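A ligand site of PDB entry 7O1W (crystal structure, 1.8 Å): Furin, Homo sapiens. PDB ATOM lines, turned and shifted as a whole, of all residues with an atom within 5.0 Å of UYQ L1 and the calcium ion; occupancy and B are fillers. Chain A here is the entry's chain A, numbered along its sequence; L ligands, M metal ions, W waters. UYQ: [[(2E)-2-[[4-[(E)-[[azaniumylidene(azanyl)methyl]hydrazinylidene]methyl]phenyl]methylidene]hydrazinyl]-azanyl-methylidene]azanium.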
ATOM      1  N   ASP A  46      -8.357  23.596  39.633  1.00  0.00           N
ATOM      2  CA  ASP A  46      -8.376  24.783  38.787  1.00  0.00           C
ATOM      3  C   ASP A  46      -7.518  25.891  39.405  1.00  0.00           C
ATOM      4  O   ASP A  46      -6.360  25.628  39.773  1.00  0.00           O
ATOM      5  CB  ASP A  46      -9.839  25.177  38.562  1.00  0.00           C
ATOM      6  CG  ASP A  46     -10.041  26.057  37.352  1.00  0.00           C
ATOM      7  OD1 ASP A  46      -9.820  27.255  37.477  1.00  0.00           O
ATOM      8  OD2 ASP A  46     -10.395  25.549  36.256  1.00  0.00           O
ATOM      9  N   ASP A  47      -8.032  27.114  39.544  1.00  0.00           N
ATOM     10  CA  ASP A  47      -7.216  28.257  39.943  1.00  0.00           C
ATOM     11  C   ASP A  47      -7.439  28.665  41.402  1.00  0.00           C
ATOM     12  O   ASP A  47      -6.976  29.739  41.816  1.00  0.00           O
ATOM     13  CB  ASP A  47      -7.463  29.476  39.037  1.00  0.00           C
ATOM     14  CG  ASP A  47      -8.914  29.905  38.993  1.00  0.00           C
ATOM     15  OD1 ASP A  47      -9.704  29.521  39.883  1.00  0.00           O
ATOM     16  OD2 ASP A  47      -9.275  30.609  38.035  1.00  0.00           O
ATOM     17  N   ASP A  84      -8.617  37.232  37.072  1.00  0.00           N
ATOM     18  CA  ASP A  84      -8.200  36.051  36.325  1.00  0.00           C
ATOM     19  C   ASP A  84      -8.500  34.751  37.061  1.00  0.00           C
ATOM     20  O   ASP A  84      -8.777  33.722  36.442  1.00  0.00           O
ATOM     21  CB  ASP A  84      -6.687  36.088  36.063  1.00  0.00           C
ATOM     22  CG  ASP A  84      -6.223  37.389  35.514  1.00  0.00           C
ATOM     23  OD1 ASP A  84      -6.126  38.358  36.297  1.00  0.00           O
ATOM     24  OD2 ASP A  84      -5.945  37.440  34.298  1.00  0.00           O
ATOM     25  N   ASN A  85      -8.352  34.747  38.381  1.00  0.00           N
ATOM     26  CA  ASN A  85      -8.438  33.501  39.147  1.00  0.00           C
ATOM     27  C   ASN A  85      -9.819  33.273  39.730  1.00  0.00           C
ATOM     28  O   ASN A  85      -9.961  32.779  40.848  1.00  0.00           O
ATOM     29  CB  ASN A  85      -7.389  33.493  40.229  1.00  0.00           C
ATOM     30  CG  ASN A  85      -6.005  33.500  39.646  1.00  0.00           C
ATOM     31  OD1 ASN A  85      -5.657  32.604  38.853  1.00  0.00           O
ATOM     32  ND2 ASN A  85      -5.224  34.529  39.966  1.00  0.00           N
ATOM     33  N   HIS A  87     -12.153  31.370  38.170  1.00  0.00           N
ATOM     34  CA  HIS A  87     -12.829  30.273  37.464  1.00  0.00           C
ATOM     35  C   HIS A  87     -13.132  29.102  38.389  1.00  0.00           C
ATOM     36  O   HIS A  87     -14.206  28.502  38.289  1.00  0.00           O
ATOM     37  CB  HIS A  87     -11.953  29.821  36.301  1.00  0.00           C
ATOM     38  CG  HIS A  87     -12.635  28.867  35.386  1.00  0.00           C
ATOM     39  ND1 HIS A  87     -12.370  27.514  35.392  1.00  0.00           N
ATOM     40  CD2 HIS A  87     -13.575  29.062  34.425  1.00  0.00           C
ATOM     41  CE1 HIS A  87     -13.123  26.914  34.482  1.00  0.00           C
ATOM     42  NE2 HIS A  87     -13.876  27.838  33.893  1.00  0.00           N
ATOM     43  N   LEU A 120      -3.619  25.845  38.782  1.00  0.00           N
ATOM     44  CA  LEU A 120      -3.411  26.464  37.476  1.00  0.00           C
ATOM     45  C   LEU A 120      -2.729  27.822  37.549  1.00  0.00           C
ATOM     46  O   LEU A 120      -2.420  28.400  36.491  1.00  0.00           O
ATOM     47  CB  LEU A 120      -4.748  26.643  36.740  1.00  0.00           C
ATOM     48  CG  LEU A 120      -5.466  25.379  36.270  1.00  0.00           C
ATOM     49  CD1 LEU A 120      -6.732  25.730  35.489  1.00  0.00           C
ATOM     50  CD2 LEU A 120      -4.567  24.450  35.451  1.00  0.00           C
ATOM     51  N   SER A 146     -10.852  20.923  33.677  1.00  0.00           N
ATOM     52  CA  SER A 146     -11.085  21.307  32.283  1.00  0.00           C
ATOM     53  C   SER A 146      -9.825  21.784  31.589  1.00  0.00           C
ATOM     54  O   SER A 146      -9.917  22.472  30.566  1.00  0.00           O
ATOM     55  CB  SER A 146     -12.163  22.415  32.184  1.00  0.00           C
ATOM     56  OG  SER A 146     -11.889  23.517  33.023  1.00  0.00           O
ATOM     57  N   TRP A 147      -8.651  21.393  32.077  1.00  0.00           N
ATOM     58  CA  TRP A 147      -7.375  21.802  31.516  1.00  0.00           C
ATOM     59  C   TRP A 147      -6.737  20.634  30.765  1.00  0.00           C
ATOM     60  O   TRP A 147      -7.156  19.483  30.861  1.00  0.00           O
ATOM     61  CB  TRP A 147      -6.445  22.303  32.627  1.00  0.00           C
ATOM     62  CG  TRP A 147      -6.497  21.541  33.908  1.00  0.00           C
ATOM     63  CD1 TRP A 147      -7.256  21.839  35.017  1.00  0.00           C
ATOM     64  CD2 TRP A 147      -5.725  20.382  34.252  1.00  0.00           C
ATOM     65  NE1 TRP A 147      -7.016  20.909  36.006  1.00  0.00           N
ATOM     66  CE2 TRP A 147      -6.091  20.002  35.562  1.00  0.00           C
ATOM     67  CE3 TRP A 147      -4.785  19.601  33.574  1.00  0.00           C
ATOM     68  CZ2 TRP A 147      -5.528  18.908  36.215  1.00  0.00           C
ATOM     69  CZ3 TRP A 147      -4.237  18.514  34.224  1.00  0.00           C
ATOM     70  CH2 TRP A 147      -4.601  18.180  35.533  1.00  0.00           C
ATOM     71  N   GLY A 148      -5.671  20.953  30.040  1.00  0.00           N
ATOM     72  CA  GLY A 148      -5.023  20.027  29.153  1.00  0.00           C
ATOM     73  C   GLY A 148      -4.276  20.805  28.097  1.00  0.00           C
ATOM     74  O   GLY A 148      -4.045  22.014  28.230  1.00  0.00           O
ATOM     75  N   PRO A 149      -3.887  20.126  27.025  1.00  0.00           N
ATOM     76  CA  PRO A 149      -3.077  20.772  25.987  1.00  0.00           C
ATOM     77  C   PRO A 149      -3.812  21.931  25.347  1.00  0.00           C
ATOM     78  O   PRO A 149      -5.042  21.989  25.319  1.00  0.00           O
ATOM     79  CB  PRO A 149      -2.823  19.653  24.969  1.00  0.00           C
ATOM     80  CG  PRO A 149      -3.879  18.617  25.249  1.00  0.00           C
ATOM     81  CD  PRO A 149      -4.153  18.704  26.721  1.00  0.00           C
ATOM     82  N   GLU A 150      -3.028  22.862  24.803  1.00  0.00           N
ATOM     83  CA  GLU A 150      -3.607  24.041  24.178  1.00  0.00           C
ATOM     84  C   GLU A 150      -4.656  23.656  23.136  1.00  0.00           C
ATOM     85  O   GLU A 150      -4.449  22.757  22.326  1.00  0.00           O
ATOM     86  CB  GLU A 150      -2.519  24.887  23.514  1.00  0.00           C
ATOM     87  CG  GLU A 150      -2.968  26.257  23.079  1.00  0.00           C
ATOM     88  N   ASP A 151      -5.794  24.350  23.176  1.00  0.00           N
ATOM     89  CA  ASP A 151      -6.874  24.133  22.221  1.00  0.00           C
ATOM     90  C   ASP A 151      -6.642  24.935  20.949  1.00  0.00           C
ATOM     91  O   ASP A 151      -7.522  25.664  20.481  1.00  0.00           O
ATOM     92  CB  ASP A 151      -8.215  24.471  22.868  1.00  0.00           C
ATOM     93  CG  ASP A 151      -8.679  23.466  23.902  1.00  0.00           C
ATOM     94  OD1 ASP A 151      -8.330  22.273  23.753  1.00  0.00           O
ATOM     95  OD2 ASP A 151      -9.460  23.827  24.823  1.00  0.00           O
ATOM     96  N   ALA A 185     -13.746  18.036  31.085  1.00  0.00           N
ATOM     97  CA  ALA A 185     -14.345  18.740  29.963  1.00  0.00           C
ATOM     98  C   ALA A 185     -13.590  18.372  28.683  1.00  0.00           C
ATOM     99  O   ALA A 185     -12.369  18.257  28.679  1.00  0.00           O
ATOM    100  CB  ALA A 185     -14.290  20.248  30.190  1.00  0.00           C
ATOM    101  N   SER A 186     -14.333  18.213  27.584  1.00  0.00           N
ATOM    102  CA  SER A 186     -13.710  17.733  26.346  1.00  0.00           C
ATOM    103  C   SER A 186     -12.913  18.791  25.592  1.00  0.00           C
ATOM    104  O   SER A 186     -12.245  18.430  24.608  1.00  0.00           O
ATOM    105  CB  SER A 186     -14.759  17.118  25.416  1.00  0.00           C
ATOM    106  OG  SER A 186     -15.797  18.040  25.131  1.00  0.00           O
ATOM    107  N   GLY A 187     -12.946  20.060  26.001  1.00  0.00           N
ATOM    108  CA  GLY A 187     -12.132  21.112  25.395  1.00  0.00           C
ATOM    109  C   GLY A 187     -12.965  22.296  24.905  1.00  0.00           C
ATOM    110  O   GLY A 187     -14.190  22.252  24.827  1.00  0.00           O
ATOM    111  N   GLY A 189     -11.791  24.105  21.886  1.00  0.00           N
ATOM    112  CA  GLY A 189     -11.082  24.446  20.663  1.00  0.00           C
ATOM    113  C   GLY A 189     -11.922  24.455  19.389  1.00  0.00           C
ATOM    114  O   GLY A 189     -11.370  24.373  18.278  1.00  0.00           O
ATOM    115  N   ASP A 194     -10.539  22.080  16.389  1.00  0.00           N
ATOM    116  CA  ASP A 194      -9.822  21.065  17.161  1.00  0.00           C
ATOM    117  C   ASP A 194     -10.670  19.797  17.250  1.00  0.00           C
ATOM    118  O   ASP A 194     -11.902  19.826  17.148  1.00  0.00           O
ATOM    119  CB  ASP A 194      -9.495  21.623  18.550  1.00  0.00           C
ATOM    120  CG  ASP A 194      -8.365  20.894  19.221  1.00  0.00           C
ATOM    121  OD1 ASP A 194      -7.851  19.904  18.635  1.00  0.00           O
ATOM    122  OD2 ASP A 194      -7.970  21.319  20.335  1.00  0.00           O
ATOM    123  N   CYS A 196     -11.030  16.387  19.661  1.00  0.00           N
ATOM    124  CA  CYS A 196     -10.575  16.250  21.049  1.00  0.00           C
ATOM    125  C   CYS A 196      -9.936  14.889  21.381  1.00  0.00           C
ATOM    126  O   CYS A 196      -9.422  14.749  22.497  1.00  0.00           O
ATOM    127  CB  CYS A 196     -11.699  16.545  22.049  1.00  0.00           C
ATOM    128  SG  CYS A 196     -13.432  16.054  21.683  1.00  0.00           S
ATOM    129  N   ASP A 199      -6.395  15.269  22.683  1.00  0.00           N
ATOM    130  CA  ASP A 199      -6.186  15.702  24.071  1.00  0.00           C
ATOM    131  C   ASP A 199      -6.212  14.433  24.917  1.00  0.00           C
ATOM    132  O   ASP A 199      -7.265  13.829  25.110  1.00  0.00           O
ATOM    133  CB  ASP A 199      -7.290  16.712  24.417  1.00  0.00           C
ATOM    134  CG  ASP A 199      -7.444  17.017  25.911  1.00  0.00           C
ATOM    135  OD1 ASP A 199      -6.802  16.379  26.773  1.00  0.00           O
ATOM    136  OD2 ASP A 199      -8.257  17.907  26.224  1.00  0.00           O
ATOM    137  N   GLU A 224     -15.629  20.799  20.803  1.00  0.00           N
ATOM    138  CA  GLU A 224     -14.837  19.864  20.030  1.00  0.00           C
ATOM    139  C   GLU A 224     -15.559  18.542  19.949  1.00  0.00           C
ATOM    140  O   GLU A 224     -16.025  18.015  20.977  1.00  0.00           O
ATOM    141  CB  GLU A 224     -13.457  19.622  20.642  1.00  0.00           C
ATOM    142  CG  GLU A 224     -12.657  20.936  20.809  1.00  0.00           C
ATOM    143  CD  GLU A 224     -11.280  20.679  21.430  1.00  0.00           C
ATOM    144  OE1 GLU A 224     -10.831  21.519  22.251  1.00  0.00           O
ATOM    145  OE2 GLU A 224     -10.655  19.637  21.073  1.00  0.00           O
HETATM  146  N1  UYQ L   1      -8.532  28.818  35.266  1.00  0.00           N
HETATM  147  C7  UYQ L   1      -7.711  21.563  27.313  1.00  0.00           C
HETATM  148  C8  UYQ L   1      -5.806  26.958  28.806  1.00  0.00           C
HETATM  149  N2  UYQ L   1      -7.157  29.962  33.833  1.00  0.00           N
HETATM  150  C9  UYQ L   1      -5.877  28.010  29.705  1.00  0.00           C
HETATM  151  C1  UYQ L   1      -6.603  28.999  31.871  1.00  0.00           C
HETATM  152  C5  UYQ L   1      -6.430  25.741  29.088  1.00  0.00           C
HETATM  153  C6  UYQ L   1      -6.444  24.678  28.089  1.00  0.00           C
HETATM  154  N3  UYQ L   1      -7.230  28.883  32.978  1.00  0.00           N
HETATM  155  C4  UYQ L   1      -7.115  25.617  30.286  1.00  0.00           C
HETATM  156  C3  UYQ L   1      -7.177  26.673  31.182  1.00  0.00           C
HETATM  157  C2  UYQ L   1      -6.558  27.884  30.912  1.00  0.00           C
HETATM  158  N4  UYQ L   1      -7.159  23.634  28.251  1.00  0.00           N
HETATM  159  N   UYQ L   1      -7.790  30.921  35.828  1.00  0.00           N
HETATM  160  C   UYQ L   1      -7.842  29.902  34.979  1.00  0.00           C
HETATM  161  N5  UYQ L   1      -6.975  22.680  27.270  1.00  0.00           N
HETATM  162  N6  UYQ L   1      -8.666  21.420  28.222  1.00  0.00           N
HETATM  163  N7  UYQ L   1      -7.385  20.576  26.507  1.00  0.00           N
HETATM  164  N1  UYQ L   2       0.303  17.802  29.079  1.00  0.00           N
HETATM  165  C7  UYQ L   2      -3.489  29.910  32.683  1.00  0.00           C
HETATM  166  C8  UYQ L   2      -2.726  24.859  32.117  1.00  0.00           C
HETATM  167  N2  UYQ L   2      -0.745  19.569  30.121  1.00  0.00           N
HETATM  168  C9  UYQ L   2      -2.496  23.497  32.146  1.00  0.00           C
HETATM  169  C1  UYQ L   2      -1.755  21.385  31.034  1.00  0.00           C
HETATM  170  C5  UYQ L   2      -2.660  25.572  30.917  1.00  0.00           C
HETATM  171  C6  UYQ L   2      -2.835  27.026  30.864  1.00  0.00           C
HETATM  172  N3  UYQ L   2      -1.294  20.826  29.993  1.00  0.00           N
HETATM  173  C4  UYQ L   2      -2.367  24.862  29.758  1.00  0.00           C
HETATM  174  C3  UYQ L   2      -2.120  23.500  29.802  1.00  0.00           C
HETATM  175  C2  UYQ L   2      -2.169  22.794  30.995  1.00  0.00           C
HETATM  176  N4  UYQ L   2      -3.094  27.723  31.905  1.00  0.00           N
HETATM  177  N   UYQ L   2      -0.187  19.709  27.886  1.00  0.00           N
HETATM  178  C   UYQ L   2      -0.200  19.028  29.014  1.00  0.00           C
HETATM  179  N5  UYQ L   2      -3.277  29.063  31.649  1.00  0.00           N
HETATM  180  N6  UYQ L   2      -3.657  31.187  32.427  1.00  0.00           N
HETATM  181  N7  UYQ L   2      -3.526  29.448  33.918  1.00  0.00           N
HETATM  182 CA    CA M   1      -8.709  20.368  22.453  1.00  0.00          CA
HETATM  183  O   HOH W   1      -6.397  20.307  23.193  1.00  0.00           O
HETATM  184  O   HOH W   2      -9.695  18.964  24.068  1.00  0.00           O
HETATM  185  O   HOH W   3      -9.635  18.771  28.254  1.00  0.00           O
HETATM  186  O   HOH W   4      -9.684  26.337  33.809  1.00  0.00           O
HETATM  187  O   HOH W   5      -7.667  18.398  21.266  1.00  0.00           O
HETATM  188  O   HOH W   6      -6.569  32.741  33.204  1.00  0.00           O
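His 87 touches UYQ L1.
CD1 of Leu 120 touches N1 of UYQ L1, at 3.6 Å.
Trp 147 touches UYQ L1.
Hydrophobic or aromatic side chains that line UYQ L1: His 87, Leu 120 and Pro 149.
Within 4 Å of UYQ L1: Asp 46, Asp 47, Asp 84, His 87, Leu 120, Ser 146, Trp 147, Gly 148, Pro 149, Asp 151 and Asp 199.
The nearest printed residue that does not touch UYQ L1 is Asn 85 (4.1 Å).
The backbone carbonyl oxygen of Leu 120 sits at hydrogen-bond distance from a nitrogen (N7) of UYQ L2.
O of Asp 84 is in hydrogen-bond range of N of UYQ L1 (3.0 Å).
A nitrogen (N5) of UYQ L1 sits close to the backbone carbonyl oxygen (O) of Gly 148, 3.2 Å away.
The backbone carbonyl oxygen (O) of Ser 146 is in hydrogen-bond range of a nitrogen (N6) of UYQ L1, at 2.9 Å.
A nitrogen (N7) of UYQ L1 lies within salt-bridge range of the side-chain carboxylate (OD2) of Asp 199.
N7 of UYQ L1 sits close to OD1 of Asp 151, 3.4 Å away.
The side-chain carboxylate of Asp 46 is in salt-bridge range of a nitrogen (N1) of UYQ L1 (3.0 Å).
N7 of UYQ L1 sits at hydrogen-bond distance from O of Pro 149, 3.0 Å away.
N of UYQ L1 lies within salt-bridge range of OD2 of Asp 47, 2.7 Å away.
Three residues have an atom within 4 Å of the calcium ion: Asp 151, Asp 194 and Glu 224.
Water W1 lies within hydrogen-bond range of O of Pro 149 (3.0 Å), O of Glu 150 (3.2 Å) and N7 of UYQ L1 (3.5 Å).
Water W2 bridges O of Ser 186 (2.7 Å) and OD2 of Asp 199 (2.8 Å).
Water W3 lies within hydrogen-bond range of OD2 of Asp 199 (2.6 Å), O of Ala 185 (2.8 Å) and N6 of UYQ L1 (2.8 Å).
Water W6 bridges N2 of UYQ L1 (2.9 Å) and N6 of UYQ L2 (3.4 Å).
Water W4 lies within hydrogen-bond range of OD2 of Asp 46 (2.7 Å), N1 of UYQ L1 (3.1 Å) and ND1 of His 87 (3.3 Å).
The calcium ion is bound by OD1 of Asp 151 (2.3 Å), water W2 (2.4 Å), OE1 of Glu 224 (2.4 Å), water W1 (2.4 Å), OD2 of Asp 194 (2.4 Å), OE2 of Glu 224 (2.5 Å) and water W5 (2.5 Å).
The calcium ion has seven donor atoms within binding distance.
The side-chain carboxylate (OE1) of Glu 224 lies close to the backbone NH (N) of Gly 189 (2.8 Å).
The side-chain carboxylate (OD2) of Asp 46 lies within hydrogen-bond range of a ring nitrogen (ND1) of His 87, 2.9 Å away.
The backbone NH (N) of Asp 194 sits at hydrogen-bond distance from the backbone carbonyl oxygen (O) of Gly 189.
The backbone NH (N) of Leu 120 is in hydrogen-bond range of the backbone carbonyl oxygen (O) of Asp 46 (2.9 Å).
The side-chain carboxylate of Asp 47 lies within hydrogen-bond range of the backbone NH of His 87 (3.0 Å).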
